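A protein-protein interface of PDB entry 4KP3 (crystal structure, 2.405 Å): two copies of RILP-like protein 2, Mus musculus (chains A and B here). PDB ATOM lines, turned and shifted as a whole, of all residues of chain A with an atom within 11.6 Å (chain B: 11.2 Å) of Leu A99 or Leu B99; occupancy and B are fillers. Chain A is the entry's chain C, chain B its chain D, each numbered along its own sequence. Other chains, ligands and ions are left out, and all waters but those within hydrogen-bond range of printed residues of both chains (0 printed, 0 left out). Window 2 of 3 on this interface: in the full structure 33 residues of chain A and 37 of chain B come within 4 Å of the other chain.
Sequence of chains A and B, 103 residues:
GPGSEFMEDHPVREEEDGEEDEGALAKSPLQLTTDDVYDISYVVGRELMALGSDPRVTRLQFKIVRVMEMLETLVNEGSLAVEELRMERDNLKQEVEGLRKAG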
ATOM      1  N   ASP A  90      -4.800 -21.832  18.085  1.00  0.00           N
ATOM      2  CA  ASP A  90      -5.290 -21.579  16.733  1.00  0.00           C
ATOM      3  C   ASP A  90      -6.442 -20.583  16.727  1.00  0.00           C
ATOM      4  O   ASP A  90      -6.529 -19.733  15.836  1.00  0.00           O
ATOM      5  CB  ASP A  90      -5.693 -22.881  16.031  1.00  0.00           C
ATOM      6  CG  ASP A  90      -4.513 -23.808  15.804  1.00  0.00           C
ATOM      7  OD1 ASP A  90      -3.364 -23.369  16.023  1.00  0.00           O
ATOM      8  OD2 ASP A  90      -4.732 -24.970  15.401  1.00  0.00           O
ATOM      9  N   ASN A  91      -7.314 -20.685  17.726  1.00  0.00           N
ATOM     10  CA  ASN A  91      -8.435 -19.758  17.860  1.00  0.00           C
ATOM     11  C   ASN A  91      -7.997 -18.319  18.136  1.00  0.00           C
ATOM     12  O   ASN A  91      -8.484 -17.385  17.500  1.00  0.00           O
ATOM     13  CB  ASN A  91      -9.429 -20.255  18.913  1.00  0.00           C
ATOM     14  CG  ASN A  91     -10.302 -21.388  18.398  1.00  0.00           C
ATOM     15  OD1 ASN A  91     -10.588 -21.468  17.201  1.00  0.00           O
ATOM     16  ND2 ASN A  91     -10.729 -22.269  19.297  1.00  0.00           N
ATOM     17  N   LEU A  92      -7.071 -18.146  19.075  1.00  0.00           N
ATOM     18  CA  LEU A  92      -6.464 -16.841  19.322  1.00  0.00           C
ATOM     19  C   LEU A  92      -5.824 -16.290  18.048  1.00  0.00           C
ATOM     20  O   LEU A  92      -5.986 -15.115  17.720  1.00  0.00           O
ATOM     21  CB  LEU A  92      -5.413 -16.938  20.427  1.00  0.00           C
ATOM     22  CG  LEU A  92      -5.914 -17.151  21.854  1.00  0.00           C
ATOM     23  CD1 LEU A  92      -4.774 -17.616  22.748  1.00  0.00           C
ATOM     24  CD2 LEU A  92      -6.529 -15.872  22.391  1.00  0.00           C
ATOM     25  N   LYS A  93      -5.100 -17.151  17.336  1.00  0.00           N
ATOM     26  CA  LYS A  93      -4.469 -16.777  16.071  1.00  0.00           C
ATOM     27  C   LYS A  93      -5.502 -16.297  15.051  1.00  0.00           C
ATOM     28  O   LYS A  93      -5.278 -15.305  14.356  1.00  0.00           O
ATOM     29  CB  LYS A  93      -3.680 -17.957  15.495  1.00  0.00           C
ATOM     30  CG  LYS A  93      -2.171 -17.827  15.603  1.00  0.00           C
ATOM     31  CD  LYS A  93      -1.480 -19.105  15.145  1.00  0.00           C
ATOM     32  CE  LYS A  93       0.033 -18.954  15.133  1.00  0.00           C
ATOM     33  NZ  LYS A  93       0.721 -20.265  14.943  1.00  0.00           N
ATOM     34  N   GLN A  94      -6.624 -17.010  14.964  1.00  0.00           N
ATOM     35  CA  GLN A  94      -7.720 -16.626  14.079  1.00  0.00           C
ATOM     36  C   GLN A  94      -8.184 -15.218  14.420  1.00  0.00           C
ATOM     37  O   GLN A  94      -8.424 -14.401  13.532  1.00  0.00           O
ATOM     38  CB  GLN A  94      -8.900 -17.598  14.207  1.00  0.00           C
ATOM     39  CG  GLN A  94      -8.673 -18.984  13.617  1.00  0.00           C
ATOM     40  CD  GLN A  94      -9.763 -19.967  14.015  1.00  0.00           C
ATOM     41  OE1 GLN A  94      -9.897 -21.039  13.423  1.00  0.00           O
ATOM     42  NE2 GLN A  94     -10.545 -19.606  15.028  1.00  0.00           N
ATOM     43  N   GLU A  95      -8.293 -14.937  15.716  1.00  0.00           N
ATOM     44  CA  GLU A  95      -8.761 -13.637  16.184  1.00  0.00           C
ATOM     45  C   GLU A  95      -7.769 -12.520  15.874  1.00  0.00           C
ATOM     46  O   GLU A  95      -8.163 -11.398  15.557  1.00  0.00           O
ATOM     47  CB  GLU A  95      -9.056 -13.673  17.683  1.00  0.00           C
ATOM     48  CG  GLU A  95      -9.664 -12.384  18.201  1.00  0.00           C
ATOM     49  CD  GLU A  95     -10.163 -12.501  19.618  1.00  0.00           C
ATOM     50  OE1 GLU A  95     -10.790 -11.536  20.099  1.00  0.00           O
ATOM     51  OE2 GLU A  95      -9.931 -13.552  20.253  1.00  0.00           O
ATOM     52  N   VAL A  96      -6.482 -12.828  15.970  1.00  0.00           N
ATOM     53  CA  VAL A  96      -5.454 -11.849  15.648  1.00  0.00           C
ATOM     54  C   VAL A  96      -5.543 -11.459  14.171  1.00  0.00           C
ATOM     55  O   VAL A  96      -5.518 -10.275  13.831  1.00  0.00           O
ATOM     56  CB  VAL A  96      -4.038 -12.361  16.002  1.00  0.00           C
ATOM     57  CG1 VAL A  96      -2.973 -11.420  15.454  1.00  0.00           C
ATOM     58  CG2 VAL A  96      -3.888 -12.513  17.511  1.00  0.00           C
ATOM     59  N   GLU A  97      -5.670 -12.457  13.301  1.00  0.00           N
ATOM     60  CA  GLU A  97      -5.793 -12.207  11.867  1.00  0.00           C
ATOM     61  C   GLU A  97      -7.042 -11.398  11.532  1.00  0.00           C
ATOM     62  O   GLU A  97      -7.003 -10.501  10.689  1.00  0.00           O
ATOM     63  CB  GLU A  97      -5.779 -13.519  11.076  1.00  0.00           C
ATOM     64  CG  GLU A  97      -4.460 -14.266  11.158  1.00  0.00           C
ATOM     65  CD  GLU A  97      -3.261 -13.333  11.069  1.00  0.00           C
ATOM     66  OE1 GLU A  97      -3.131 -12.617  10.054  1.00  0.00           O
ATOM     67  OE2 GLU A  97      -2.455 -13.308  12.024  1.00  0.00           O
ATOM     68  N   GLY A  98      -8.144 -11.712  12.202  1.00  0.00           N
ATOM     69  CA  GLY A  98      -9.403 -11.032  11.958  1.00  0.00           C
ATOM     70  C   GLY A  98      -9.428  -9.580  12.399  1.00  0.00           C
ATOM     71  O   GLY A  98     -10.050  -8.743  11.745  1.00  0.00           O
ATOM     72  N   LEU A  99      -8.757  -9.275  13.506  1.00  0.00           N
ATOM     73  CA  LEU A  99      -8.746  -7.912  14.036  1.00  0.00           C
ATOM     74  C   LEU A  99      -7.800  -6.988  13.265  1.00  0.00           C
ATOM     75  O   LEU A  99      -7.898  -5.765  13.366  1.00  0.00           O
ATOM     76  CB  LEU A  99      -8.412  -7.911  15.531  1.00  0.00           C
ATOM     77  CG  LEU A  99      -9.467  -8.552  16.442  1.00  0.00           C
ATOM     78  CD1 LEU A  99      -9.028  -8.545  17.901  1.00  0.00           C
ATOM     79  CD2 LEU A  99     -10.814  -7.858  16.282  1.00  0.00           C
ATOM     80  N   ARG A 100      -6.894  -7.575  12.487  1.00  0.00           N
ATOM     81  CA  ARG A 100      -5.948  -6.797  11.690  1.00  0.00           C
ATOM     82  C   ARG A 100      -6.329  -6.754  10.212  1.00  0.00           C
ATOM     83  O   ARG A 100      -7.285  -7.402   9.785  1.00  0.00           O
ATOM     84  CB  ARG A 100      -4.529  -7.347  11.860  1.00  0.00           C
ATOM     85  CG  ARG A 100      -3.987  -7.181  13.265  1.00  0.00           C
ATOM     86  CD  ARG A 100      -2.547  -7.644  13.387  1.00  0.00           C
ATOM     87  NE  ARG A 100      -1.945  -7.122  14.610  1.00  0.00           N
ATOM     88  CZ  ARG A 100      -0.785  -7.532  15.112  1.00  0.00           C
ATOM     89  NH1 ARG A 100      -0.093  -8.484  14.501  1.00  0.00           N
ATOM     90  NH2 ARG A 100      -0.323  -6.993  16.230  1.00  0.00           N
ATOM     91  N   ASN B  91       1.307 -15.489  25.147  1.00  0.00           N
ATOM     92  CA  ASN B  91       1.666 -14.348  24.314  1.00  0.00           C
ATOM     93  C   ASN B  91       0.525 -13.912  23.394  1.00  0.00           C
ATOM     94  O   ASN B  91       0.267 -12.718  23.234  1.00  0.00           O
ATOM     95  CB  ASN B  91       2.935 -14.639  23.506  1.00  0.00           C
ATOM     96  CG  ASN B  91       4.194 -14.637  24.365  1.00  0.00           C
ATOM     97  OD1 ASN B  91       4.333 -13.825  25.284  1.00  0.00           O
ATOM     98  ND2 ASN B  91       5.117 -15.546  24.066  1.00  0.00           N
ATOM     99  N   LEU B  92      -0.163 -14.885  22.805  1.00  0.00           N
ATOM    100  CA  LEU B  92      -1.293 -14.597  21.928  1.00  0.00           C
ATOM    101  C   LEU B  92      -2.442 -13.930  22.680  1.00  0.00           C
ATOM    102  O   LEU B  92      -3.094 -13.030  22.152  1.00  0.00           O
ATOM    103  CB  LEU B  92      -1.774 -15.870  21.232  1.00  0.00           C
ATOM    104  CG  LEU B  92      -0.977 -16.257  19.987  1.00  0.00           C
ATOM    105  CD1 LEU B  92      -1.282 -17.686  19.550  1.00  0.00           C
ATOM    106  CD2 LEU B  92      -1.260 -15.271  18.860  1.00  0.00           C
ATOM    107  N   LYS B  93      -2.679 -14.360  23.915  1.00  0.00           N
ATOM    108  CA  LYS B  93      -3.724 -13.751  24.735  1.00  0.00           C
ATOM    109  C   LYS B  93      -3.409 -12.295  25.077  1.00  0.00           C
ATOM    110  O   LYS B  93      -4.311 -11.461  25.168  1.00  0.00           O
ATOM    111  CB  LYS B  93      -3.990 -14.570  26.005  1.00  0.00           C
ATOM    112  CG  LYS B  93      -5.216 -15.470  25.888  1.00  0.00           C
ATOM    113  CD  LYS B  93      -5.505 -16.243  27.166  1.00  0.00           C
ATOM    114  CE  LYS B  93      -6.812 -17.022  27.036  1.00  0.00           C
ATOM    115  NZ  LYS B  93      -7.042 -17.968  28.165  1.00  0.00           N
ATOM    116  N   GLN B  94      -2.130 -11.982  25.249  1.00  0.00           N
ATOM    117  CA  GLN B  94      -1.737 -10.599  25.495  1.00  0.00           C
ATOM    118  C   GLN B  94      -1.927  -9.747  24.243  1.00  0.00           C
ATOM    119  O   GLN B  94      -2.394  -8.608  24.319  1.00  0.00           O
ATOM    120  CB  GLN B  94      -0.292 -10.522  25.992  1.00  0.00           C
ATOM    121  CG  GLN B  94      -0.047 -11.353  27.237  1.00  0.00           C
ATOM    122  CD  GLN B  94       1.180 -10.918  28.008  1.00  0.00           C
ATOM    123  OE1 GLN B  94       2.226 -10.627  27.428  1.00  0.00           O
ATOM    124  NE2 GLN B  94       1.054 -10.864  29.330  1.00  0.00           N
ATOM    125  N   GLU B  95      -1.575 -10.306  23.090  1.00  0.00           N
ATOM    126  CA  GLU B  95      -1.753  -9.601  21.825  1.00  0.00           C
ATOM    127  C   GLU B  95      -3.236  -9.334  21.532  1.00  0.00           C
ATOM    128  O   GLU B  95      -3.607  -8.218  21.174  1.00  0.00           O
ATOM    129  CB  GLU B  95      -1.092 -10.375  20.678  1.00  0.00           C
ATOM    130  CG  GLU B  95      -1.260  -9.729  19.310  1.00  0.00           C
ATOM    131  CD  GLU B  95      -0.499 -10.462  18.220  1.00  0.00           C
ATOM    132  OE1 GLU B  95      -0.460  -9.959  17.075  1.00  0.00           O
ATOM    133  OE2 GLU B  95       0.063 -11.539  18.508  1.00  0.00           O
ATOM    134  N   VAL B  96      -4.075 -10.355  21.698  1.00  0.00           N
ATOM    135  CA  VAL B  96      -5.517 -10.222  21.477  1.00  0.00           C
ATOM    136  C   VAL B  96      -6.147  -9.153  22.374  1.00  0.00           C
ATOM    137  O   VAL B  96      -7.001  -8.379  21.933  1.00  0.00           O
ATOM    138  CB  VAL B  96      -6.255 -11.569  21.680  1.00  0.00           C
ATOM    139  CG1 VAL B  96      -7.760 -11.358  21.765  1.00  0.00           C
ATOM    140  CG2 VAL B  96      -5.914 -12.538  20.561  1.00  0.00           C
ATOM    141  N   GLU B  97      -5.721  -9.110  23.632  1.00  0.00           N
ATOM    142  CA  GLU B  97      -6.225  -8.120  24.579  1.00  0.00           C
ATOM    143  C   GLU B  97      -5.938  -6.694  24.111  1.00  0.00           C
ATOM    144  O   GLU B  97      -6.802  -5.818  24.189  1.00  0.00           O
ATOM    145  CB  GLU B  97      -5.629  -8.361  25.967  1.00  0.00           C
ATOM    146  CG  GLU B  97      -5.841  -7.218  26.945  1.00  0.00           C
ATOM    147  CD  GLU B  97      -5.227  -7.503  28.299  1.00  0.00           C
ATOM    148  OE1 GLU B  97      -4.977  -8.690  28.598  1.00  0.00           O
ATOM    149  OE2 GLU B  97      -4.995  -6.541  29.063  1.00  0.00           O
ATOM    150  N   GLY B  98      -4.726  -6.467  23.615  1.00  0.00           N
ATOM    151  CA  GLY B  98      -4.354  -5.160  23.106  1.00  0.00           C
ATOM    152  C   GLY B  98      -5.146  -4.784  21.870  1.00  0.00           C
ATOM    153  O   GLY B  98      -5.601  -3.647  21.732  1.00  0.00           O
ATOM    154  N   LEU B  99      -5.319  -5.748  20.971  1.00  0.00           N
ATOM    155  CA  LEU B  99      -6.049  -5.517  19.729  1.00  0.00           C
ATOM    156  C   LEU B  99      -7.534  -5.266  19.977  1.00  0.00           C
ATOM    157  O   LEU B  99      -8.213  -4.654  19.152  1.00  0.00           O
ATOM    158  CB  LEU B  99      -5.844  -6.684  18.760  1.00  0.00           C
ATOM    159  CG  LEU B  99      -4.396  -6.883  18.305  1.00  0.00           C
ATOM    160  CD1 LEU B  99      -4.252  -8.135  17.455  1.00  0.00           C
ATOM    161  CD2 LEU B  99      -3.892  -5.657  17.552  1.00  0.00           C
ATOM    162  N   ARG B 100      -8.035  -5.736  21.117  1.00  0.00           N
ATOM    163  CA  ARG B 100      -9.419  -5.479  21.502  1.00  0.00           C
ATOM    164  C   ARG B 100      -9.619  -4.040  21.973  1.00  0.00           C
ATOM    165  O   ARG B 100     -10.703  -3.476  21.821  1.00  0.00           O
ATOM    166  CB  ARG B 100      -9.877  -6.468  22.573  1.00  0.00           C
ATOM    167  CG  ARG B 100     -10.239  -7.832  22.018  1.00  0.00           C
ATOM    168  CD  ARG B 100     -10.379  -8.865  23.117  1.00  0.00           C
ATOM    169  NE  ARG B 100     -10.942 -10.114  22.614  1.00  0.00           N
ATOM    170  CZ  ARG B 100     -11.004 -11.245  23.311  1.00  0.00           C
ATOM    171  NH1 ARG B 100     -10.526 -11.295  24.547  1.00  0.00           N
ATOM    172  NH2 ARG B 100     -11.538 -12.331  22.768  1.00  0.00           N
ATOM    173  N   LYS B 101      -8.570  -3.448  22.535  1.00  0.00           N
ATOM    174  CA  LYS B 101      -8.613  -2.049  22.946  1.00  0.00           C
ATOM    175  C   LYS B 101      -8.193  -1.135  21.798  1.00  0.00           C
ATOM    176  O   LYS B 101      -8.858  -1.072  20.764  1.00  0.00           O
ATOM    177  CB  LYS B 101      -7.708  -1.811  24.156  1.00  0.00           C
ATOM    178  CG  LYS B 101      -7.972  -2.737  25.331  1.00  0.00           C
ATOM    179  CD  LYS B 101      -7.056  -2.410  26.498  1.00  0.00           C
ATOM    180  CE  LYS B 101      -7.243  -3.389  27.643  1.00  0.00           C
ATOM    181  NZ  LYS B 101      -6.414  -3.017  28.823  1.00  0.00           N
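Among the printed residues, merely in contact across the chains: Val A96 with Glu B95 (3.3 Å), Glu A95 with Val B96 (3.4 Å), Val A96 with Val B96 (3.7 Å), Leu A92 with Lys B93 (3.8 Å), Leu A99 with Leu B99 (3.8 Å), Leu A92 with Leu B92 (3.8 Å), Arg A100 with Leu B99 (3.8 Å) and Leu A92 with Val B96 (3.8 Å).
Of the 11 printed residues of chain A, 5 touch a printed residue of chain B. Of the 11 printed residues of chain B, 6 touch a printed residue of chain A. Printed residues of chain B that touch a printed residue of chain A: Leu B92, Lys B93, Glu B95, Val B96, Leu B99 and Arg B100. Hydrophobic or aromatic side chains of chain B within 4 Å of the printed part of chain A: Leu B92, Val B96 and Leu B99. Along chain B the printed residues that touch a printed residue of chain A span positions 92 to 100.
OE1 of Glu A95 lies within salt-bridge range of NH2 of Arg B100 (2.9 Å). The side-chain carboxylate (OE1) of Glu B95 lies within salt-bridge range of the guanidinium group (NH1) of Arg A100.
Of chain B, only Leu B99 comes within 4 Å of Leu A99. Leu B99 touches two residues of chain A. Of chain B, only Val B96 (3.4 Å) and Arg B100 (2.9 Å) come within 4 Å of Glu A95. No residue of chain B comes within 4 Å of Gly A98. Of chain B, only Glu B95 and Leu B99 come within 4 Å of Arg A100. Of chain A, only Val A96 (3.3 Å) and Arg A100 (3.0 Å) come within 4 Å of Glu B95. Val B96 touches just these residues of chain A: Leu A92 (3.8 Å), Glu A95 (3.4 Å) and Val A96 (3.7 Å). No residue of chain A comes within 4 Å of Gly B98. Printed residues of chain A within 4 Å of Lys B93: Leu A92 (3.8 Å). Of the printed residues of chain B, Leu A92 touches Leu B92 (3.8 Å), Lys B93 (3.8 Å) and Val B96 (3.8 Å). Of the printed residues of chain A, Leu B92 touches Leu A92 (3.8 Å). Lys B101 touches none of the printed residues of chain A. Gln B94 touches none of the printed residues of chain A. The nearest residue of chain B that does not touch Leu A99 is Arg B100 (4.4 Å). The nearest printed residue of chain A that does not touch Lys B93 is Val A96 (6.8 Å).
Leu A92 touches Lys B93, but with the chains exchanged Lys A93 does not touch Leu B92 (4.05 Å). Glu A95 touches Val B96, and with the chains exchanged Val A96 touches Glu B95. Glu A95 touches Arg B100, and with the chains exchanged Arg A100 touches Glu B95. Val A96 touches its own counterpart, Val B96. 10 positions are printed for both chains. Of the 10 pairs that touch across the chains among the printed residues, 7 have their exchanged pair printed and touching as well.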
